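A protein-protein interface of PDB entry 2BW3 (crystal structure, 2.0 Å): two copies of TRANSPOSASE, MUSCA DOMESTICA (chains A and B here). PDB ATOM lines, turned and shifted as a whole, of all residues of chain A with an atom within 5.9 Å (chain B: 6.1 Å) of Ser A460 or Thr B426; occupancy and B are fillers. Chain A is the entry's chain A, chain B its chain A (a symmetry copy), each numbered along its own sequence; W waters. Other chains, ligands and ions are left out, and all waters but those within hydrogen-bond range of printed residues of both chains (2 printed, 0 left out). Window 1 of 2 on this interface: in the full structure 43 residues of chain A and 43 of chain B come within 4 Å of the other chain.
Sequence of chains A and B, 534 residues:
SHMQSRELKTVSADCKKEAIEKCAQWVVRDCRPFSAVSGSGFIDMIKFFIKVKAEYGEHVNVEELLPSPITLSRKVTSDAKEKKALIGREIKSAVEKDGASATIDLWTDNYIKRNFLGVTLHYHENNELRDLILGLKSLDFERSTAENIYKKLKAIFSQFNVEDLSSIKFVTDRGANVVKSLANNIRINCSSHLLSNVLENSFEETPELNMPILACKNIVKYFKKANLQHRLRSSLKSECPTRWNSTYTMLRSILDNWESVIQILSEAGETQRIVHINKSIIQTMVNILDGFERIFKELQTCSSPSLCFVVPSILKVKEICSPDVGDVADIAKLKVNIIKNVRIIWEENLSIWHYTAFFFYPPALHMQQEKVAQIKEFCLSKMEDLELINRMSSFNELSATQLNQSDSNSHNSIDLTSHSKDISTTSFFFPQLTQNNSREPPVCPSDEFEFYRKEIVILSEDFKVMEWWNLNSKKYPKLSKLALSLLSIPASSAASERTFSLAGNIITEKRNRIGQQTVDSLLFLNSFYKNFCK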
ATOM      1  N   ARG A 294      21.243 -13.289  -0.912  1.00  0.00           N
ATOM      2  CA  ARG A 294      21.885 -13.906  -2.053  1.00  0.00           C
ATOM      3  C   ARG A 294      23.397 -13.783  -1.934  1.00  0.00           C
ATOM      4  O   ARG A 294      24.141 -14.672  -2.380  1.00  0.00           O
ATOM      5  CB  ARG A 294      21.378 -13.269  -3.349  1.00  0.00           C
ATOM      6  CG  ARG A 294      21.988 -13.857  -4.645  1.00  0.00           C
ATOM      7  CD  ARG A 294      21.396 -15.189  -5.040  1.00  0.00           C
ATOM      8  NE  ARG A 294      22.034 -15.770  -6.225  1.00  0.00           N
ATOM      9  CZ  ARG A 294      21.591 -15.652  -7.480  1.00  0.00           C
ATOM     10  NH1 ARG A 294      20.495 -14.942  -7.769  1.00  0.00           N
ATOM     11  NH2 ARG A 294      22.178 -16.351  -8.446  1.00  0.00           N
ATOM     12  N   PHE A 309      34.175 -13.858  -5.978  1.00  0.00           N
ATOM     13  CA  PHE A 309      32.980 -13.034  -5.927  1.00  0.00           C
ATOM     14  C   PHE A 309      32.923 -12.117  -4.715  1.00  0.00           C
ATOM     15  O   PHE A 309      31.931 -11.412  -4.536  1.00  0.00           O
ATOM     16  CB  PHE A 309      31.710 -13.895  -5.985  1.00  0.00           C
ATOM     17  CG  PHE A 309      31.542 -14.651  -7.294  1.00  0.00           C
ATOM     18  CD1 PHE A 309      31.082 -15.963  -7.304  1.00  0.00           C
ATOM     19  CD2 PHE A 309      31.847 -14.048  -8.509  1.00  0.00           C
ATOM     20  CE1 PHE A 309      30.927 -16.665  -8.513  1.00  0.00           C
ATOM     21  CE2 PHE A 309      31.694 -14.741  -9.720  1.00  0.00           C
ATOM     22  CZ  PHE A 309      31.234 -16.049  -9.710  1.00  0.00           C
ATOM     23  N   TYR A 361      39.147 -14.017 -12.505  1.00  0.00           N
ATOM     24  CA  TYR A 361      37.855 -14.291 -13.117  1.00  0.00           C
ATOM     25  C   TYR A 361      38.047 -13.487 -14.420  1.00  0.00           C
ATOM     26  O   TYR A 361      37.823 -12.277 -14.461  1.00  0.00           O
ATOM     27  CB  TYR A 361      36.745 -13.722 -12.230  1.00  0.00           C
ATOM     28  CG  TYR A 361      35.363 -14.100 -12.680  1.00  0.00           C
ATOM     29  CD1 TYR A 361      34.832 -15.346 -12.360  1.00  0.00           C
ATOM     30  CD2 TYR A 361      34.583 -13.222 -13.453  1.00  0.00           C
ATOM     31  CE1 TYR A 361      33.557 -15.728 -12.797  1.00  0.00           C
ATOM     32  CE2 TYR A 361      33.298 -13.603 -13.895  1.00  0.00           C
ATOM     33  CZ  TYR A 361      32.802 -14.849 -13.564  1.00  0.00           C
ATOM     34  OH  TYR A 361      31.546 -15.266 -13.997  1.00  0.00           O
ATOM     35  N   PRO A 363      36.406 -12.804 -17.338  1.00  0.00           N
ATOM     36  CA  PRO A 363      35.474 -11.822 -17.906  1.00  0.00           C
ATOM     37  C   PRO A 363      35.508 -10.463 -17.228  1.00  0.00           C
ATOM     38  O   PRO A 363      35.008  -9.490 -17.782  1.00  0.00           O
ATOM     39  CB  PRO A 363      34.114 -12.497 -17.730  1.00  0.00           C
ATOM     40  CG  PRO A 363      34.449 -13.962 -17.805  1.00  0.00           C
ATOM     41  CD  PRO A 363      35.692 -14.022 -16.928  1.00  0.00           C
ATOM     42  N   ILE A 458      34.450 -13.494 -22.711  1.00  0.00           N
ATOM     43  CA  ILE A 458      33.053 -13.119 -22.670  1.00  0.00           C
ATOM     44  C   ILE A 458      32.313 -13.703 -21.497  1.00  0.00           C
ATOM     45  O   ILE A 458      32.428 -14.894 -21.210  1.00  0.00           O
ATOM     46  CB  ILE A 458      32.323 -13.535 -24.000  1.00  0.00           C
ATOM     47  CG1 ILE A 458      33.124 -13.047 -25.205  1.00  0.00           C
ATOM     48  CG2 ILE A 458      30.941 -12.879 -24.074  1.00  0.00           C
ATOM     49  CD1 ILE A 458      33.362 -11.552 -25.192  1.00  0.00           C
ATOM     50  N   LEU A 459      31.574 -12.849 -20.801  1.00  0.00           N
ATOM     51  CA  LEU A 459      30.764 -13.297 -19.689  1.00  0.00           C
ATOM     52  C   LEU A 459      29.492 -13.963 -20.251  1.00  0.00           C
ATOM     53  O   LEU A 459      28.750 -13.346 -21.011  1.00  0.00           O
ATOM     54  CB  LEU A 459      30.337 -12.098 -18.809  1.00  0.00           C
ATOM     55  CG  LEU A 459      29.434 -12.506 -17.641  1.00  0.00           C
ATOM     56  CD1 LEU A 459      30.295 -13.327 -16.667  1.00  0.00           C
ATOM     57  CD2 LEU A 459      28.830 -11.287 -16.910  1.00  0.00           C
ATOM     58  N   SER A 460      29.225 -15.197 -19.842  1.00  0.00           N
ATOM     59  CA  SER A 460      28.018 -15.912 -20.245  1.00  0.00           C
ATOM     60  C   SER A 460      27.523 -16.490 -18.926  1.00  0.00           C
ATOM     61  O   SER A 460      28.331 -16.680 -18.006  1.00  0.00           O
ATOM     62  CB  SER A 460      28.342 -17.024 -21.256  1.00  0.00           C
ATOM     63  OG  SER A 460      29.151 -18.051 -20.701  1.00  0.00           O
ATOM     64  N   GLU A 461      26.230 -16.794 -18.802  1.00  0.00           N
ATOM     65  CA  GLU A 461      25.757 -17.332 -17.526  1.00  0.00           C
ATOM     66  C   GLU A 461      26.261 -18.739 -17.192  1.00  0.00           C
ATOM     67  O   GLU A 461      26.334 -19.125 -16.018  1.00  0.00           O
ATOM     68  CB  GLU A 461      24.239 -17.199 -17.362  1.00  0.00           C
ATOM     69  CG  GLU A 461      23.379 -18.106 -18.194  1.00  0.00           C
ATOM     70  CD  GLU A 461      21.935 -18.069 -17.726  1.00  0.00           C
ATOM     71  OE1 GLU A 461      21.303 -16.990 -17.809  1.00  0.00           O
ATOM     72  OE2 GLU A 461      21.444 -19.114 -17.244  1.00  0.00           O
ATOM     73  N   ASP A 462      26.662 -19.489 -18.210  1.00  0.00           N
ATOM     74  CA  ASP A 462      27.196 -20.820 -17.965  1.00  0.00           C
ATOM     75  C   ASP A 462      28.734 -20.755 -17.847  1.00  0.00           C
ATOM     76  O   ASP A 462      29.404 -21.785 -17.927  1.00  0.00           O
ATOM     77  CB  ASP A 462      26.782 -21.791 -19.076  1.00  0.00           C
ATOM     78  CG  ASP A 462      27.287 -21.375 -20.445  1.00  0.00           C
ATOM     79  OD1 ASP A 462      27.659 -22.276 -21.233  1.00  0.00           O
ATOM     80  OD2 ASP A 462      27.312 -20.160 -20.746  1.00  0.00           O
ATOM     81  N   PHE A 463      29.287 -19.550 -17.687  1.00  0.00           N
ATOM     82  CA  PHE A 463      30.738 -19.401 -17.543  1.00  0.00           C
ATOM     83  C   PHE A 463      31.201 -20.057 -16.231  1.00  0.00           C
ATOM     84  O   PHE A 463      30.619 -19.821 -15.183  1.00  0.00           O
ATOM     85  CB  PHE A 463      31.157 -17.923 -17.573  1.00  0.00           C
ATOM     86  CG  PHE A 463      32.653 -17.722 -17.508  1.00  0.00           C
ATOM     87  CD1 PHE A 463      33.446 -17.939 -18.641  1.00  0.00           C
ATOM     88  CD2 PHE A 463      33.285 -17.444 -16.294  1.00  0.00           C
ATOM     89  CE1 PHE A 463      34.847 -17.899 -18.559  1.00  0.00           C
ATOM     90  CE2 PHE A 463      34.689 -17.406 -16.208  1.00  0.00           C
ATOM     91  CZ  PHE A 463      35.466 -17.633 -17.323  1.00  0.00           C
ATOM     92  N   SER B 424      20.663 -15.517 -12.714  1.00  0.00           N
ATOM     93  CA  SER B 424      21.903 -16.278 -12.680  1.00  0.00           C
ATOM     94  C   SER B 424      22.920 -15.577 -11.771  1.00  0.00           C
ATOM     95  O   SER B 424      22.835 -14.374 -11.511  1.00  0.00           O
ATOM     96  CB  SER B 424      22.469 -16.417 -14.096  1.00  0.00           C
ATOM     97  OG  SER B 424      22.738 -15.143 -14.643  1.00  0.00           O
ATOM     98  N   THR B 425      23.944 -16.315 -11.382  1.00  0.00           N
ATOM     99  CA  THR B 425      24.959 -15.765 -10.517  1.00  0.00           C
ATOM    100  C   THR B 425      25.736 -14.692 -11.258  1.00  0.00           C
ATOM    101  O   THR B 425      25.991 -13.627 -10.719  1.00  0.00           O
ATOM    102  CB  THR B 425      25.812 -16.902  -9.997  1.00  0.00           C
ATOM    103  OG1 THR B 425      24.961 -17.719  -9.174  1.00  0.00           O
ATOM    104  CG2 THR B 425      27.021 -16.388  -9.184  1.00  0.00           C
ATOM    105  N   THR B 426      25.986 -14.911 -12.545  1.00  0.00           N
ATOM    106  CA  THR B 426      26.720 -13.920 -13.316  1.00  0.00           C
ATOM    107  C   THR B 426      25.913 -12.626 -13.489  1.00  0.00           C
ATOM    108  O   THR B 426      26.473 -11.550 -13.526  1.00  0.00           O
ATOM    109  CB  THR B 426      27.150 -14.501 -14.707  1.00  0.00           C
ATOM    110  OG1 THR B 426      26.002 -15.018 -15.390  1.00  0.00           O
ATOM    111  CG2 THR B 426      28.167 -15.644 -14.521  1.00  0.00           C
ATOM    112  N   SER B 427      24.589 -12.727 -13.604  1.00  0.00           N
ATOM    113  CA  SER B 427      23.766 -11.523 -13.775  1.00  0.00           C
ATOM    114  C   SER B 427      23.657 -10.775 -12.465  1.00  0.00           C
ATOM    115  O   SER B 427      23.563  -9.542 -12.434  1.00  0.00           O
ATOM    116  CB  SER B 427      22.358 -11.884 -14.281  1.00  0.00           C
ATOM    117  OG  SER B 427      22.410 -12.395 -15.606  1.00  0.00           O
ATOM    118  N   PHE B 428      23.591 -11.536 -11.384  1.00  0.00           N
ATOM    119  CA  PHE B 428      23.517 -10.939 -10.057  1.00  0.00           C
ATOM    120  C   PHE B 428      24.775 -10.090  -9.806  1.00  0.00           C
ATOM    121  O   PHE B 428      24.699  -8.882  -9.534  1.00  0.00           O
ATOM    122  CB  PHE B 428      23.394 -12.038  -8.996  1.00  0.00           C
ATOM    123  CG  PHE B 428      23.251 -11.501  -7.595  1.00  0.00           C
ATOM    124  CD1 PHE B 428      22.069 -10.869  -7.197  1.00  0.00           C
ATOM    125  CD2 PHE B 428      24.301 -11.592  -6.687  1.00  0.00           C
ATOM    126  CE1 PHE B 428      21.936 -10.335  -5.903  1.00  0.00           C
ATOM    127  CE2 PHE B 428      24.172 -11.060  -5.384  1.00  0.00           C
ATOM    128  CZ  PHE B 428      23.004 -10.440  -4.998  1.00  0.00           C
ATOM    129  N   PHE B 429      25.939 -10.709  -9.948  1.00  0.00           N
ATOM    130  CA  PHE B 429      27.183  -9.991  -9.693  1.00  0.00           C
ATOM    131  C   PHE B 429      27.693  -9.053 -10.756  1.00  0.00           C
ATOM    132  O   PHE B 429      28.429  -8.119 -10.447  1.00  0.00           O
ATOM    133  CB  PHE B 429      28.283 -10.975  -9.348  1.00  0.00           C
ATOM    134  CG  PHE B 429      28.121 -11.588  -8.001  1.00  0.00           C
ATOM    135  CD1 PHE B 429      28.112 -12.961  -7.849  1.00  0.00           C
ATOM    136  CD2 PHE B 429      28.015 -10.779  -6.870  1.00  0.00           C
ATOM    137  CE1 PHE B 429      28.001 -13.540  -6.577  1.00  0.00           C
ATOM    138  CE2 PHE B 429      27.905 -11.337  -5.605  1.00  0.00           C
ATOM    139  CZ  PHE B 429      27.898 -12.729  -5.454  1.00  0.00           C
ATOM    140  N   PHE B 430      27.359  -9.315 -12.018  1.00  0.00           N
ATOM    141  CA  PHE B 430      27.819  -8.455 -13.100  1.00  0.00           C
ATOM    142  C   PHE B 430      26.627  -7.944 -13.916  1.00  0.00           C
ATOM    143  O   PHE B 430      26.457  -8.324 -15.087  1.00  0.00           O
ATOM    144  CB  PHE B 430      28.777  -9.239 -13.984  1.00  0.00           C
ATOM    145  CG  PHE B 430      29.954  -9.803 -13.229  1.00  0.00           C
ATOM    146  CD1 PHE B 430      29.988 -11.142 -12.885  1.00  0.00           C
ATOM    147  CD2 PHE B 430      30.993  -8.966 -12.813  1.00  0.00           C
ATOM    148  CE1 PHE B 430      31.043 -11.666 -12.124  1.00  0.00           C
ATOM    149  CE2 PHE B 430      32.058  -9.476 -12.051  1.00  0.00           C
ATOM    150  CZ  PHE B 430      32.073 -10.833 -11.707  1.00  0.00           C
ATOM    151  N   PRO B 431      25.785  -7.092 -13.302  1.00  0.00           N
ATOM    152  CA  PRO B 431      24.594  -6.534 -13.966  1.00  0.00           C
ATOM    153  C   PRO B 431      24.914  -5.655 -15.171  1.00  0.00           C
ATOM    154  O   PRO B 431      24.236  -5.719 -16.198  1.00  0.00           O
ATOM    155  CB  PRO B 431      23.915  -5.742 -12.842  1.00  0.00           C
ATOM    156  CG  PRO B 431      25.073  -5.342 -11.940  1.00  0.00           C
ATOM    157  CD  PRO B 431      25.893  -6.598 -11.913  1.00  0.00           C
ATOM    158  N   THR B 434      26.288  -7.876 -17.959  1.00  0.00           N
ATOM    159  CA  THR B 434      25.154  -8.656 -18.418  1.00  0.00           C
ATOM    160  C   THR B 434      24.212  -7.864 -19.344  1.00  0.00           C
ATOM    161  O   THR B 434      23.869  -8.345 -20.424  1.00  0.00           O
ATOM    162  CB  THR B 434      24.398  -9.253 -17.221  1.00  0.00           C
ATOM    163  OG1 THR B 434      25.248 -10.200 -16.569  1.00  0.00           O
ATOM    164  CG2 THR B 434      23.114  -9.937 -17.662  1.00  0.00           C
ATOM    165  N   ASN B 437      25.947  -7.209 -22.748  1.00  0.00           N
ATOM    166  CA  ASN B 437      25.922  -8.389 -23.608  1.00  0.00           C
ATOM    167  C   ASN B 437      24.559  -8.662 -24.221  1.00  0.00           C
ATOM    168  O   ASN B 437      24.470  -9.245 -25.300  1.00  0.00           O
ATOM    169  CB  ASN B 437      26.398  -9.618 -22.839  1.00  0.00           C
ATOM    170  CG  ASN B 437      27.823  -9.476 -22.351  1.00  0.00           C
ATOM    171  OD1 ASN B 437      28.560  -8.569 -22.773  1.00  0.00           O
ATOM    172  ND2 ASN B 437      28.219 -10.354 -21.437  1.00  0.00           N
ATOM    173  N   LYS B 474      31.449 -19.735 -26.911  1.00  0.00           N
ATOM    174  CA  LYS B 474      30.867 -18.411 -26.648  1.00  0.00           C
ATOM    175  C   LYS B 474      31.629 -17.375 -27.421  1.00  0.00           C
ATOM    176  O   LYS B 474      31.075 -16.382 -27.898  1.00  0.00           O
ATOM    177  CB  LYS B 474      30.921 -18.048 -25.156  1.00  0.00           C
ATOM    178  CG  LYS B 474      30.394 -19.116 -24.236  1.00  0.00           C
ATOM    179  CD  LYS B 474      28.927 -19.376 -24.452  1.00  0.00           C
ATOM    180  CE  LYS B 474      28.557 -20.687 -23.791  1.00  0.00           C
ATOM    181  NZ  LYS B 474      27.081 -20.864 -23.702  1.00  0.00           N
HETATM  182  O   HOH W   1      31.366  -9.952 -21.128  1.00  0.00           O
HETATM  183  O   HOH W   2      25.939 -17.799 -13.469  1.00  0.00           O
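Ile A458 touches none of the printed residues of chain B.
Of the printed residues of chain B, Leu A459 touches Thr B426 (3.8 Å), Phe B430 (3.6 Å), Thr B434 (3.8 Å) and Asn B437 (3.1 Å).
Of chain B, only Thr B426 and Lys B474 come within 4 Å of Ser A460.
Thr B426 touches four residues of chain A.
Printed residues of chain A within 4 Å of Phe B428: Arg A294.
Printed residues of chain A within 4 Å of Phe B429: Phe A309.
Printed residues of chain A within 4 Å of Thr B434: Leu A459.
The nearest residue of chain B that does not touch Ser A460 is Asn B437 (5.2 Å).
The nearest residue of chain A that does not touch Thr B426 is Phe A463 (4.8 Å).
The nearest printed residue of chain B that does not touch Leu A459 is Ser B427 (5.6 Å).
Water W2 lies within hydrogen-bond range of O of Glu A461 (2.9 Å), N of Thr B426 (3.0 Å) and N of Thr B425 (3.2 Å).
Water W1 lies within hydrogen-bond range of the backbone NH of Leu A459 (2.9 Å) and the side-chain amide nitrogen of Asn B437 (3.2 Å).
Hydrophobic or aromatic side chains of chain B that line the printed part of chain A: Phe B428, Phe B429 and Phe B430.
Of the 10 printed residues of chain A, 7 touch a printed residue of chain B.
Along chain A the printed residues that touch a printed residue of chain B span positions 294 to 462.
Arg A294 touches Ser B424.
CZ of Phe B428 touches CG of Arg A294 (3.6 Å).
Phe A309 touches Phe B430.
Tyr A361 touches Thr B426.
Tyr A361 touches Phe B430.
Leu A459 touches Thr B426.
Leu A459 touches Thr B434.
Thr B426 touches Ser A460 (CG2 to O, 3.6 Å).
Ser A460 touches Lys B474.
CB of Glu A461 touches OG of Ser B424 (3.7 Å).
No position is printed for both chains.
Of the 17 pairs that touch across the chains among the printed residues, none has its exchanged pair printed and touching as well.
ND2 of Asn B437 lies within hydrogen-bond range of O of Leu A459 (3.1 Å).
The side-chain hydroxyl (OG1) of Thr B425 is in hydrogen-bond range of the guanidinium group (NH2) of Arg A294, 3.2 Å away.
OD1 of Asp A462 is in salt-bridge range of NZ of Lys B474.
The side-chain hydroxyl (OG) of Ser B424 lies within hydrogen-bond range of the side-chain hydroxyl (OG1) of Thr B426 (3.4 Å).
The backbone NH (N) of Phe A463 is in hydrogen-bond range of the side-chain hydroxyl (OG) of Ser A460 (3.4 Å).
The side-chain hydroxyl (OG) of Ser B424 is in hydrogen-bond range of the side-chain hydroxyl (OG) of Ser B427.
The side-chain hydroxyl (OG) of Ser A460 sits at hydrogen-bond distance from the side-chain carboxylate (OD2) of Asp A462 (2.8 Å).
The backbone carbonyl oxygen (O) of Phe B430 sits at hydrogen-bond distance from the side-chain hydroxyl (OG1) of Thr B434 (2.7 Å).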
